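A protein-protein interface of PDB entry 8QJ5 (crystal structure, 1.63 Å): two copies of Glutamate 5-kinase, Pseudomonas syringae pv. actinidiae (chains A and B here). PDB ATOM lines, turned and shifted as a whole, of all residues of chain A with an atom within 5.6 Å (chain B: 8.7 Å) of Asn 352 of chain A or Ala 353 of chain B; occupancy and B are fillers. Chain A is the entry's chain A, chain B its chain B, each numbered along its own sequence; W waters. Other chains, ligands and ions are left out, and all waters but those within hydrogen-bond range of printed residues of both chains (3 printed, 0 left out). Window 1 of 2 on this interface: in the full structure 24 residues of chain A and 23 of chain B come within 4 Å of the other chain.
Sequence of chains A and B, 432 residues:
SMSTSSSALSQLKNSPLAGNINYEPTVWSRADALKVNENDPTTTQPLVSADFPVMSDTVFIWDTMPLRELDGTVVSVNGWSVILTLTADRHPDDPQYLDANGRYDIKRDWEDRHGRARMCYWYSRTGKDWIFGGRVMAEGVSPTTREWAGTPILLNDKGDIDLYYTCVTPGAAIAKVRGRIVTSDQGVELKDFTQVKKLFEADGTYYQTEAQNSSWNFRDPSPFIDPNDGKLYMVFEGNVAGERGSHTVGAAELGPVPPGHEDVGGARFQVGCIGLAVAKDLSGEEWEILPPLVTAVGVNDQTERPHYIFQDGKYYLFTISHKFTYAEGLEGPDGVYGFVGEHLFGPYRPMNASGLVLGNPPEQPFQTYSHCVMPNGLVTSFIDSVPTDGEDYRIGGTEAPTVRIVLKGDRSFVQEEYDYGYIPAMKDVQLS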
ATOM      1  N   THR A  43      36.278  12.218  -6.562  1.00  0.00           N
ATOM      2  CA  THR A  43      35.767  11.257  -7.541  1.00  0.00           C
ATOM      3  C   THR A  43      36.640  11.236  -8.804  1.00  0.00           C
ATOM      4  O   THR A  43      36.135  10.970  -9.884  1.00  0.00           O
ATOM      5  CB  THR A  43      34.264  11.450  -7.859  1.00  0.00           C
ATOM      6  OG1 THR A  43      34.049  12.766  -8.398  1.00  0.00           O
ATOM      7  CG2 THR A  43      33.376  11.202  -6.660  1.00  0.00           C
ATOM      8  N   PRO A 350      21.229   7.850  -7.909  1.00  0.00           N
ATOM      9  CA  PRO A 350      22.575   8.008  -8.466  1.00  0.00           C
ATOM     10  C   PRO A 350      23.607   8.298  -7.382  1.00  0.00           C
ATOM     11  O   PRO A 350      23.373   9.134  -6.516  1.00  0.00           O
ATOM     12  CB  PRO A 350      22.533   9.231  -9.383  1.00  0.00           C
ATOM     13  CG  PRO A 350      21.073   9.648  -9.399  1.00  0.00           C
ATOM     14  CD  PRO A 350      20.336   8.984  -8.235  1.00  0.00           C
ATOM     15  N   MET A 351      24.728   7.583  -7.417  1.00  0.00           N
ATOM     16  CA  MET A 351      25.829   7.814  -6.479  1.00  0.00           C
ATOM     17  C   MET A 351      26.356   9.245  -6.613  1.00  0.00           C
ATOM     18  O   MET A 351      26.496   9.741  -7.733  1.00  0.00           O
ATOM     19  CB  MET A 351      26.987   6.839  -6.739  1.00  0.00           C
ATOM     20  CG  MET A 351      26.639   5.426  -6.250  1.00  0.00           C
ATOM     21  SD  MET A 351      26.662   5.321  -4.455  1.00  0.00           S
ATOM     22  CE  MET A 351      28.418   5.482  -4.126  1.00  0.00           C
ATOM     23  N   ASN A 352      26.694   9.884  -5.469  1.00  0.00           N
ATOM     24  CA  ASN A 352      27.220  11.244  -5.447  1.00  0.00           C
ATOM     25  C   ASN A 352      26.300  12.259  -6.138  1.00  0.00           C
ATOM     26  O   ASN A 352      26.789  13.253  -6.712  1.00  0.00           O
ATOM     27  CB  ASN A 352      28.599  11.301  -6.068  1.00  0.00           C
ATOM     28  CG  ASN A 352      29.567  10.437  -5.298  1.00  0.00           C
ATOM     29  OD1 ASN A 352      29.665  10.570  -4.076  1.00  0.00           O
ATOM     30  ND2 ASN A 352      30.203   9.462  -5.969  1.00  0.00           N
ATOM     31  N   ALA A 353      25.000  11.925  -6.183  1.00  0.00           N
ATOM     32  CA  ALA A 353      23.915  12.714  -6.770  1.00  0.00           C
ATOM     33  C   ALA A 353      23.909  12.710  -8.310  1.00  0.00           C
ATOM     34  O   ALA A 353      22.828  12.743  -8.906  1.00  0.00           O
ATOM     35  CB  ALA A 353      23.899  14.166  -6.253  1.00  0.00           C
ATOM     36  N   SER A 354      25.088  12.801  -8.959  1.00  0.00           N
ATOM     37  CA  SER A 354      25.166  12.858 -10.411  1.00  0.00           C
ATOM     38  C   SER A 354      25.210  11.448 -11.040  1.00  0.00           C
ATOM     39  O   SER A 354      24.831  11.280 -12.224  1.00  0.00           O
ATOM     40  CB  SER A 354      26.419  13.623 -10.796  1.00  0.00           C
ATOM     41  OG  SER A 354      27.577  12.872 -10.435  1.00  0.00           O
ATOM     42  N   GLY A 355      25.702  10.476 -10.253  1.00  0.00           N
ATOM     43  CA  GLY A 355      26.004   9.137 -10.755  1.00  0.00           C
ATOM     44  C   GLY A 355      27.505   8.878 -10.832  1.00  0.00           C
ATOM     45  O   GLY A 355      27.948   7.706 -10.884  1.00  0.00           O
ATOM     46  N   LEU A 356      28.309   9.955 -10.902  1.00  0.00           N
ATOM     47  CA  LEU A 356      29.730   9.715 -11.146  1.00  0.00           C
ATOM     48  C   LEU A 356      30.450   9.238  -9.890  1.00  0.00           C
ATOM     49  O   LEU A 356      30.339   9.892  -8.870  1.00  0.00           O
ATOM     50  CB  LEU A 356      30.400  11.000 -11.677  1.00  0.00           C
ATOM     51  CG  LEU A 356      31.935  10.904 -11.780  1.00  0.00           C
ATOM     52  CD1 LEU A 356      32.354   9.944 -12.932  1.00  0.00           C
ATOM     53  CD2 LEU A 356      32.512  12.274 -12.153  1.00  0.00           C
ATOM     54  N   VAL A 357      31.209   8.135 -10.005  1.00  0.00           N
ATOM     55  CA  VAL A 357      31.925   7.529  -8.870  1.00  0.00           C
ATOM     56  C   VAL A 357      33.425   7.787  -9.060  1.00  0.00           C
ATOM     57  O   VAL A 357      34.103   8.217  -8.108  1.00  0.00           O
ATOM     58  CB  VAL A 357      31.635   6.013  -8.758  1.00  0.00           C
ATOM     59  CG1 VAL A 357      32.627   5.309  -7.795  1.00  0.00           C
ATOM     60  CG2 VAL A 357      30.194   5.763  -8.325  1.00  0.00           C
ATOM     61  N   ASP A 410      25.222   7.009   0.103  1.00  0.00           N
ATOM     62  CA  ASP A 410      25.016   7.141  -1.337  1.00  0.00           C
ATOM     63  C   ASP A 410      26.192   7.892  -1.946  1.00  0.00           C
ATOM     64  O   ASP A 410      26.055   8.445  -3.029  1.00  0.00           O
ATOM     65  CB  ASP A 410      23.689   7.873  -1.627  1.00  0.00           C
ATOM     66  CG  ASP A 410      22.464   7.070  -1.198  1.00  0.00           C
ATOM     67  OD1 ASP A 410      22.636   5.979  -0.636  1.00  0.00           O
ATOM     68  OD2 ASP A 410      21.316   7.557  -1.447  1.00  0.00           O
ATOM     69  N   ARG A 411      27.331   7.953  -1.237  1.00  0.00           N
ATOM     70  CA  ARG A 411      28.475   8.722  -1.741  1.00  0.00           C
ATOM     71  C   ARG A 411      29.715   7.825  -1.775  1.00  0.00           C
ATOM     72  O   ARG A 411      29.751   6.797  -1.097  1.00  0.00           O
ATOM     73  CB  ARG A 411      28.797   9.909  -0.815  1.00  0.00           C
ATOM     74  CG  ARG A 411      27.682  10.973  -0.782  1.00  0.00           C
ATOM     75  CD  ARG A 411      26.902  10.805   0.513  1.00  0.00           C
ATOM     76  NE  ARG A 411      27.677  11.406   1.574  1.00  0.00           N
ATOM     77  CZ  ARG A 411      27.505  11.135   2.868  1.00  0.00           C
ATOM     78  NH1 ARG A 411      26.567  10.290   3.273  1.00  0.00           N
ATOM     79  NH2 ARG A 411      28.291  11.751   3.755  1.00  0.00           N
ATOM     80  N   SER A 412      30.698   8.251  -2.575  1.00  0.00           N
ATOM     81  CA  SER A 412      31.985   7.544  -2.606  1.00  0.00           C
ATOM     82  C   SER A 412      33.130   8.550  -2.523  1.00  0.00           C
ATOM     83  O   SER A 412      32.988   9.708  -2.887  1.00  0.00           O
ATOM     84  CB  SER A 412      32.070   6.698  -3.890  1.00  0.00           C
ATOM     85  OG  SER A 412      32.192   7.504  -5.074  1.00  0.00           O
ATOM     86  N   TRP B  28      29.010  17.219   9.077  1.00  0.00           N
ATOM     87  CA  TRP B  28      29.315  17.679   7.731  1.00  0.00           C
ATOM     88  C   TRP B  28      30.827  17.754   7.624  1.00  0.00           C
ATOM     89  O   TRP B  28      31.414  18.572   8.332  1.00  0.00           O
ATOM     90  CB  TRP B  28      28.623  19.043   7.502  1.00  0.00           C
ATOM     91  CG  TRP B  28      28.724  19.544   6.100  1.00  0.00           C
ATOM     92  CD1 TRP B  28      28.774  18.784   4.964  1.00  0.00           C
ATOM     93  CD2 TRP B  28      28.756  20.920   5.670  1.00  0.00           C
ATOM     94  NE1 TRP B  28      28.853  19.606   3.859  1.00  0.00           N
ATOM     95  CE2 TRP B  28      28.767  20.912   4.258  1.00  0.00           C
ATOM     96  CE3 TRP B  28      28.657  22.162   6.325  1.00  0.00           C
ATOM     97  CZ2 TRP B  28      28.875  22.088   3.511  1.00  0.00           C
ATOM     98  CZ3 TRP B  28      28.665  23.334   5.582  1.00  0.00           C
ATOM     99  CH2 TRP B  28      28.765  23.292   4.179  1.00  0.00           C
ATOM    100  N   SER B  29      31.463  16.795   6.891  1.00  0.00           N
ATOM    101  CA  SER B  29      32.925  16.725   6.962  1.00  0.00           C
ATOM    102  C   SER B  29      33.594  17.575   5.881  1.00  0.00           C
ATOM    103  O   SER B  29      32.940  17.984   4.922  1.00  0.00           O
ATOM    104  CB  SER B  29      33.433  15.298   6.837  1.00  0.00           C
ATOM    105  OG  SER B  29      33.182  14.851   5.499  1.00  0.00           O
ATOM    106  N   ALA B  31      35.624  16.255   3.710  1.00  0.00           N
ATOM    107  CA  ALA B  31      35.517  15.459   2.473  1.00  0.00           C
ATOM    108  C   ALA B  31      34.167  15.717   1.759  1.00  0.00           C
ATOM    109  O   ALA B  31      34.103  15.800   0.523  1.00  0.00           O
ATOM    110  CB  ALA B  31      35.645  13.971   2.819  1.00  0.00           C
ATOM    111  N   ASP B  32      33.097  15.891   2.546  1.00  0.00           N
ATOM    112  CA  ASP B  32      31.782  16.232   1.967  1.00  0.00           C
ATOM    113  C   ASP B  32      31.899  17.591   1.254  1.00  0.00           C
ATOM    114  O   ASP B  32      31.425  17.780   0.121  1.00  0.00           O
ATOM    115  CB  ASP B  32      30.698  16.381   3.031  1.00  0.00           C
ATOM    116  CG  ASP B  32      30.307  15.124   3.785  1.00  0.00           C
ATOM    117  OD1 ASP B  32      30.437  13.997   3.220  1.00  0.00           O
ATOM    118  OD2 ASP B  32      29.859  15.258   4.942  1.00  0.00           O
ATOM    119  N   ALA B  33      32.518  18.565   1.936  1.00  0.00           N
ATOM    120  CA  ALA B  33      32.622  19.912   1.390  1.00  0.00           C
ATOM    121  C   ALA B  33      33.501  19.991   0.144  1.00  0.00           C
ATOM    122  O   ALA B  33      33.360  20.919  -0.644  1.00  0.00           O
ATOM    123  CB  ALA B  33      33.097  20.910   2.458  1.00  0.00           C
ATOM    124  N   LEU B  34      34.435  19.035  -0.041  1.00  0.00           N
ATOM    125  CA  LEU B  34      35.258  19.071  -1.222  1.00  0.00           C
ATOM    126  C   LEU B  34      34.427  18.709  -2.464  1.00  0.00           C
ATOM    127  O   LEU B  34      34.887  18.971  -3.570  1.00  0.00           O
ATOM    128  CB  LEU B  34      36.371  18.011  -1.098  1.00  0.00           C
ATOM    129  CG  LEU B  34      37.496  18.392  -0.116  1.00  0.00           C
ATOM    130  CD1 LEU B  34      38.484  17.201   0.019  1.00  0.00           C
ATOM    131  CD2 LEU B  34      38.235  19.630  -0.668  1.00  0.00           C
ATOM    132  N   LYS B  35      33.248  18.143  -2.283  1.00  0.00           N
ATOM    133  CA  LYS B  35      32.391  17.870  -3.431  1.00  0.00           C
ATOM    134  C   LYS B  35      31.560  19.103  -3.849  1.00  0.00           C
ATOM    135  O   LYS B  35      30.794  19.037  -4.839  1.00  0.00           O
ATOM    136  CB  LYS B  35      31.364  16.798  -3.012  1.00  0.00           C
ATOM    137  CG  LYS B  35      31.922  15.395  -2.799  1.00  0.00           C
ATOM    138  CD  LYS B  35      30.746  14.389  -2.478  1.00  0.00           C
ATOM    139  CE  LYS B  35      31.284  12.989  -2.261  1.00  0.00           C
ATOM    140  NZ  LYS B  35      32.009  12.464  -3.455  1.00  0.00           N
ATOM    141  N   VAL B  36      31.650  20.228  -3.117  1.00  0.00           N
ATOM    142  CA  VAL B  36      30.824  21.403  -3.467  1.00  0.00           C
ATOM    143  C   VAL B  36      31.211  21.889  -4.861  1.00  0.00           C
ATOM    144  O   VAL B  36      32.381  22.080  -5.170  1.00  0.00           O
ATOM    145  CB  VAL B  36      30.973  22.536  -2.402  1.00  0.00           C
ATOM    146  CG1 VAL B  36      30.383  23.868  -2.890  1.00  0.00           C
ATOM    147  CG2 VAL B  36      30.276  22.117  -1.101  1.00  0.00           C
ATOM    148  N   ASN B  37      30.199  22.078  -5.742  1.00  0.00           N
ATOM    149  CA  ASN B  37      30.420  22.505  -7.120  1.00  0.00           C
ATOM    150  C   ASN B  37      29.694  23.837  -7.315  1.00  0.00           C
ATOM    151  O   ASN B  37      28.466  23.831  -7.373  1.00  0.00           O
ATOM    152  CB  ASN B  37      29.858  21.448  -8.079  1.00  0.00           C
ATOM    153  CG  ASN B  37      30.102  21.807  -9.535  1.00  0.00           C
ATOM    154  OD1 ASN B  37      30.763  22.820  -9.849  1.00  0.00           O
ATOM    155  ND2 ASN B  37      29.598  20.957 -10.425  1.00  0.00           N
ATOM    156  N   ASP B  40      27.333  24.150 -10.865  1.00  0.00           N
ATOM    157  CA  ASP B  40      26.309  23.184 -11.234  1.00  0.00           C
ATOM    158  C   ASP B  40      25.021  23.929 -11.610  1.00  0.00           C
ATOM    159  O   ASP B  40      24.437  24.617 -10.777  1.00  0.00           O
ATOM    160  CB  ASP B  40      26.082  22.252 -10.009  1.00  0.00           C
ATOM    161  CG  ASP B  40      25.068  21.132 -10.187  1.00  0.00           C
ATOM    162  OD1 ASP B  40      24.146  21.244 -11.063  1.00  0.00           O
ATOM    163  OD2 ASP B  40      25.216  20.101  -9.483  1.00  0.00           O
ATOM    164  N   THR B  43      21.965  23.746  -9.221  1.00  0.00           N
ATOM    165  CA  THR B  43      21.993  24.275  -7.864  1.00  0.00           C
ATOM    166  C   THR B  43      22.505  25.723  -7.864  1.00  0.00           C
ATOM    167  O   THR B  43      23.106  26.168  -6.898  1.00  0.00           O
ATOM    168  CB  THR B  43      22.797  23.352  -6.921  1.00  0.00           C
ATOM    169  OG1 THR B  43      24.140  23.270  -7.397  1.00  0.00           O
ATOM    170  CG2 THR B  43      22.146  21.982  -6.755  1.00  0.00           C
ATOM    171  N   GLY B 338      21.885  21.978   2.735  1.00  0.00           N
ATOM    172  CA  GLY B 338      20.819  21.170   3.308  1.00  0.00           C
ATOM    173  C   GLY B 338      21.267  19.757   3.660  1.00  0.00           C
ATOM    174  O   GLY B 338      22.212  19.232   3.097  1.00  0.00           O
ATOM    175  N   PHE B 339      20.520  19.134   4.586  1.00  0.00           N
ATOM    176  CA  PHE B 339      20.751  17.805   5.097  1.00  0.00           C
ATOM    177  C   PHE B 339      19.384  17.126   5.170  1.00  0.00           C
ATOM    178  O   PHE B 339      18.383  17.793   5.432  1.00  0.00           O
ATOM    179  CB  PHE B 339      21.414  17.883   6.485  1.00  0.00           C
ATOM    180  CG  PHE B 339      22.730  18.619   6.424  1.00  0.00           C
ATOM    181  CD1 PHE B 339      23.901  17.954   6.129  1.00  0.00           C
ATOM    182  CD2 PHE B 339      22.759  19.992   6.586  1.00  0.00           C
ATOM    183  CE1 PHE B 339      25.089  18.667   5.971  1.00  0.00           C
ATOM    184  CE2 PHE B 339      23.931  20.706   6.442  1.00  0.00           C
ATOM    185  CZ  PHE B 339      25.099  20.032   6.129  1.00  0.00           C
ATOM    186  N   VAL B 340      19.348  15.816   4.876  1.00  0.00           N
ATOM    187  CA  VAL B 340      18.061  15.129   4.776  1.00  0.00           C
ATOM    188  C   VAL B 340      18.114  13.829   5.579  1.00  0.00           C
ATOM    189  O   VAL B 340      19.132  13.132   5.610  1.00  0.00           O
ATOM    190  CB  VAL B 340      17.688  14.919   3.285  1.00  0.00           C
ATOM    191  CG1 VAL B 340      18.768  14.169   2.516  1.00  0.00           C
ATOM    192  CG2 VAL B 340      16.331  14.199   3.164  1.00  0.00           C
ATOM    193  N   ARG B 349      21.911  13.134   5.920  1.00  0.00           N
ATOM    194  CA  ARG B 349      22.887  13.030   4.844  1.00  0.00           C
ATOM    195  C   ARG B 349      22.898  14.360   4.091  1.00  0.00           C
ATOM    196  O   ARG B 349      21.914  15.085   4.034  1.00  0.00           O
ATOM    197  CB  ARG B 349      22.459  11.922   3.870  1.00  0.00           C
ATOM    198  CG  ARG B 349      21.823  10.774   4.632  1.00  0.00           C
ATOM    199  CD  ARG B 349      21.004   9.929   3.755  1.00  0.00           C
ATOM    200  NE  ARG B 349      19.689  10.260   3.264  1.00  0.00           N
ATOM    201  CZ  ARG B 349      18.571   9.881   3.839  1.00  0.00           C
ATOM    202  NH1 ARG B 349      18.586   9.343   5.042  1.00  0.00           N
ATOM    203  NH2 ARG B 349      17.433  10.056   3.203  1.00  0.00           N
ATOM    204  N   PRO B 350      24.047  14.774   3.531  1.00  0.00           N
ATOM    205  CA  PRO B 350      24.119  16.065   2.844  1.00  0.00           C
ATOM    206  C   PRO B 350      23.367  16.020   1.513  1.00  0.00           C
ATOM    207  O   PRO B 350      23.551  15.092   0.708  1.00  0.00           O
ATOM    208  CB  PRO B 350      25.602  16.310   2.610  1.00  0.00           C
ATOM    209  CG  PRO B 350      26.245  14.927   2.753  1.00  0.00           C
ATOM    210  CD  PRO B 350      25.311  14.018   3.545  1.00  0.00           C
ATOM    211  N   MET B 351      22.558  17.056   1.282  1.00  0.00           N
ATOM    212  CA  MET B 351      21.813  17.191   0.032  1.00  0.00           C
ATOM    213  C   MET B 351      22.771  17.295  -1.145  1.00  0.00           C
ATOM    214  O   MET B 351      23.789  17.983  -1.045  1.00  0.00           O
ATOM    215  CB  MET B 351      20.912  18.430   0.032  1.00  0.00           C
ATOM    216  CG  MET B 351      19.704  18.245   0.945  1.00  0.00           C
ATOM    217  SD  MET B 351      18.483  17.156   0.200  1.00  0.00           S
ATOM    218  CE  MET B 351      17.898  18.135  -1.183  1.00  0.00           C
ATOM    219  N   ASN B 352      22.408  16.646  -2.273  1.00  0.00           N
ATOM    220  CA  ASN B 352      23.215  16.708  -3.486  1.00  0.00           C
ATOM    221  C   ASN B 352      24.658  16.234  -3.247  1.00  0.00           C
ATOM    222  O   ASN B 352      25.573  16.706  -3.924  1.00  0.00           O
ATOM    223  CB  ASN B 352      23.234  18.128  -4.028  1.00  0.00           C
ATOM    224  CG  ASN B 352      21.839  18.532  -4.459  1.00  0.00           C
ATOM    225  OD1 ASN B 352      21.186  17.779  -5.202  1.00  0.00           O
ATOM    226  ND2 ASN B 352      21.345  19.676  -3.969  1.00  0.00           N
ATOM    227  N   ALA B 353      24.835  15.387  -2.215  1.00  0.00           N
ATOM    228  CA  ALA B 353      26.113  14.787  -1.808  1.00  0.00           C
ATOM    229  C   ALA B 353      27.075  15.764  -1.107  1.00  0.00           C
ATOM    230  O   ALA B 353      27.774  15.353  -0.167  1.00  0.00           O
ATOM    231  CB  ALA B 353      26.845  14.089  -2.970  1.00  0.00           C
ATOM    232  N   SER B 354      27.157  17.024  -1.577  1.00  0.00           N
ATOM    233  CA  SER B 354      28.081  17.995  -0.992  1.00  0.00           C
ATOM    234  C   SER B 354      27.453  18.785   0.171  1.00  0.00           C
ATOM    235  O   SER B 354      28.192  19.302   1.046  1.00  0.00           O
ATOM    236  CB  SER B 354      28.503  18.984  -2.072  1.00  0.00           C
ATOM    237  OG  SER B 354      27.357  19.759  -2.473  1.00  0.00           O
ATOM    238  N   GLY B 355      26.118  18.889   0.118  1.00  0.00           N
ATOM    239  CA  GLY B 355      25.337  19.744   1.011  1.00  0.00           C
ATOM    240  C   GLY B 355      24.775  20.968   0.308  1.00  0.00           C
ATOM    241  O   GLY B 355      23.802  21.581   0.785  1.00  0.00           O
ATOM    242  N   LEU B 356      25.368  21.343  -0.832  1.00  0.00           N
ATOM    243  CA  LEU B 356      24.884  22.569  -1.459  1.00  0.00           C
ATOM    244  C   LEU B 356      23.540  22.374  -2.172  1.00  0.00           C
ATOM    245  O   LEU B 356      23.414  21.489  -3.005  1.00  0.00           O
ATOM    246  CB  LEU B 356      25.960  23.072  -2.454  1.00  0.00           C
ATOM    247  CG  LEU B 356      25.527  24.285  -3.286  1.00  0.00           C
ATOM    248  CD1 LEU B 356      25.389  25.527  -2.380  1.00  0.00           C
ATOM    249  CD2 LEU B 356      26.560  24.627  -4.375  1.00  0.00           C
ATOM    250  N   VAL B 357      22.583  23.274  -1.885  1.00  0.00           N
ATOM    251  CA  VAL B 357      21.225  23.239  -2.442  1.00  0.00           C
ATOM    252  C   VAL B 357      21.077  24.380  -3.470  1.00  0.00           C
ATOM    253  O   VAL B 357      20.605  24.169  -4.611  1.00  0.00           O
ATOM    254  CB  VAL B 357      20.153  23.304  -1.326  1.00  0.00           C
ATOM    255  CG1 VAL B 357      18.760  23.597  -1.912  1.00  0.00           C
ATOM    256  CG2 VAL B 357      20.084  21.986  -0.546  1.00  0.00           C
ATOM    257  N   ASP B 410      17.339  12.766  -2.026  1.00  0.00           N
ATOM    258  CA  ASP B 410      18.389  13.470  -1.335  1.00  0.00           C
ATOM    259  C   ASP B 410      18.964  14.525  -2.273  1.00  0.00           C
ATOM    260  O   ASP B 410      20.080  14.984  -2.036  1.00  0.00           O
ATOM    261  CB  ASP B 410      19.466  12.493  -0.827  1.00  0.00           C
ATOM    262  CG  ASP B 410      18.971  11.547   0.270  1.00  0.00           C
ATOM    263  OD1 ASP B 410      17.764  11.564   0.631  1.00  0.00           O
ATOM    264  OD2 ASP B 410      19.803  10.764   0.756  1.00  0.00           O
ATOM    265  N   ARG B 411      18.244  14.879  -3.346  1.00  0.00           N
ATOM    266  CA  ARG B 411      18.761  15.866  -4.301  1.00  0.00           C
ATOM    267  C   ARG B 411      17.759  17.011  -4.511  1.00  0.00           C
ATOM    268  O   ARG B 411      16.578  16.875  -4.164  1.00  0.00           O
ATOM    269  CB  ARG B 411      18.981  15.210  -5.675  1.00  0.00           C
ATOM    270  CG  ARG B 411      20.027  14.091  -5.660  1.00  0.00           C
ATOM    271  CD  ARG B 411      19.340  12.724  -5.682  1.00  0.00           C
ATOM    272  NE  ARG B 411      18.922  12.502  -7.056  1.00  0.00           N
ATOM    273  CZ  ARG B 411      17.989  11.622  -7.409  1.00  0.00           C
ATOM    274  NH1 ARG B 411      17.407  10.848  -6.501  1.00  0.00           N
ATOM    275  NH2 ARG B 411      17.659  11.519  -8.686  1.00  0.00           N
ATOM    276  N   SER B 412      18.273  18.113  -5.077  1.00  0.00           N
ATOM    277  CA  SER B 412      17.395  19.243  -5.376  1.00  0.00           C
ATOM    278  C   SER B 412      17.742  19.796  -6.764  1.00  0.00           C
ATOM    279  O   SER B 412      18.855  19.655  -7.260  1.00  0.00           O
ATOM    280  CB  SER B 412      17.563  20.319  -4.289  1.00  0.00           C
ATOM    281  OG  SER B 412      18.823  21.002  -4.409  1.00  0.00           O
HETATM  282  O   HOH W   1      20.273  13.735  -9.067  1.00  0.00           O
HETATM  283  O   HOH W   2      19.580   8.102   0.564  1.00  0.00           O
HETATM  284  O   HOH W   3      29.389  13.411   0.791  1.00  0.00           O
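The side-chain amide oxygen (OD1) of Asn 352 of chain A sits at hydrogen-bond distance from the side-chain amino group (NZ) of Lys 35 of chain B (3.1 Å).
The side-chain carboxylate (OD1) of Asp 32 of chain B is in salt-bridge range of the guanidinium group (NH2) of Arg 411 of chain A.
The backbone carbonyl oxygen (O) of Ser 412 of chain A sits at hydrogen-bond distance from the side-chain amino group (NZ) of Lys 35 of chain B (3.0 Å).
ND2 of Asn 352 of chain A lies within hydrogen-bond range of O of Leu 356 of chain A (2.9 Å).
The backbone NH of Asn 352 of chain A is in hydrogen-bond range of the backbone carbonyl oxygen of Asp 410 of chain A.
ND2 of Asn 352 of chain A is in hydrogen-bond range of OG of Ser 412 of chain A.
ND2 of Asn 352 of chain B is in hydrogen-bond range of O of Leu 356 of chain B.
The backbone NH of Asn 352 of chain B sits at hydrogen-bond distance from the backbone carbonyl oxygen of Asp 410 of chain B.
ND2 of Asn 352 of chain B sits at hydrogen-bond distance from OG of Ser 412 of chain B, at 2.9 Å.
Among the printed residues, pairs that only touch across the chains: Pro 350 of chain A with Arg 411 of chain B (3.6 Å), Arg 411 of chain A with Pro 350 of chain B (3.7 Å), Asn 352 of chain A with Ala 353 of chain B (3.7 Å), Thr 43 of chain A with Lys 35 of chain B (3.7 Å), Ala 353 of chain A with Asn 352 of chain B (3.7 Å), Arg 411 of chain A with Ala 353 of chain B (3.9 Å) and Ala 353 of chain A with Arg 411 of chain B (3.9 Å).
Asn 352 of chain A touches just these residues of chain B: Lys 35 and Ala 353.
Printed residues of chain A within 4 Å of Ala 353 of chain B: Asn 352 and Arg 411.
Of the printed residues of chain B, Ser 412 of chain A touches Lys 35 (3.0 Å).
Of the printed residues of chain A, Asp 32 of chain B touches Arg 411.
Of the printed residues of chain A, Asn 352 of chain B touches Ala 353.
The nearest residue of chain B that does not touch Asn 352 of chain A is Asn 352 of chain B (4.6 Å).
Of the 26 printed residues of chain B, 6 touch a printed residue of chain A.
Hydrophobic or aromatic side chains of chain B within 4 Å of the printed part of chain A: Pro 350 and Ala 353.
Along chain B the printed residues that touch a printed residue of chain A span positions 32 to 411.
Of the 12 printed residues of chain A, 6 touch a printed residue of chain B.
Hydrophobic or aromatic side chains of chain A within 4 Å of the printed part of chain B: Pro 350 and Ala 353.
Among the printed residues, 10 pairs touch across the chains.
Pro 350 of chain A touches Arg 411 of chain B, and with the chains exchanged Arg 411 of chain A touches Pro 350 of chain B.
Asn 352 of chain A touches Ala 353 of chain B, and with the chains exchanged Ala 353 of chain A touches Asn 352 of chain B.
Ala 353 of chain A touches Arg 411 of chain B, and with the chains exchanged Arg 411 of chain A touches Ala 353 of chain B.
Positions printed for both chains: 43, 350, 351, 352, 353, 354, 355, 356, 357, 410, 411 and 412.
Of the 10 pairs that touch across the chains among the printed residues, 6 have their exchanged pair printed and touching as well.
Water W2 lies within hydrogen-bond range of OD2 of Asp 410 of chain B (2.7 Å), OD2 of Asp 410 of chain A (2.7 Å) and NE of Arg 349 of chain B (3.5 Å).
Water W3 lies within hydrogen-bond range of O of Ala 353 of chain B (2.7 Å), OD1 of Asp 32 of chain B (2.7 Å) and NE of Arg 411 of chain A (2.8 Å).
Water W1 bridges NE of Arg 411 of chain B (2.7 Å) and O of Ala 353 of chain A (2.7 Å).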
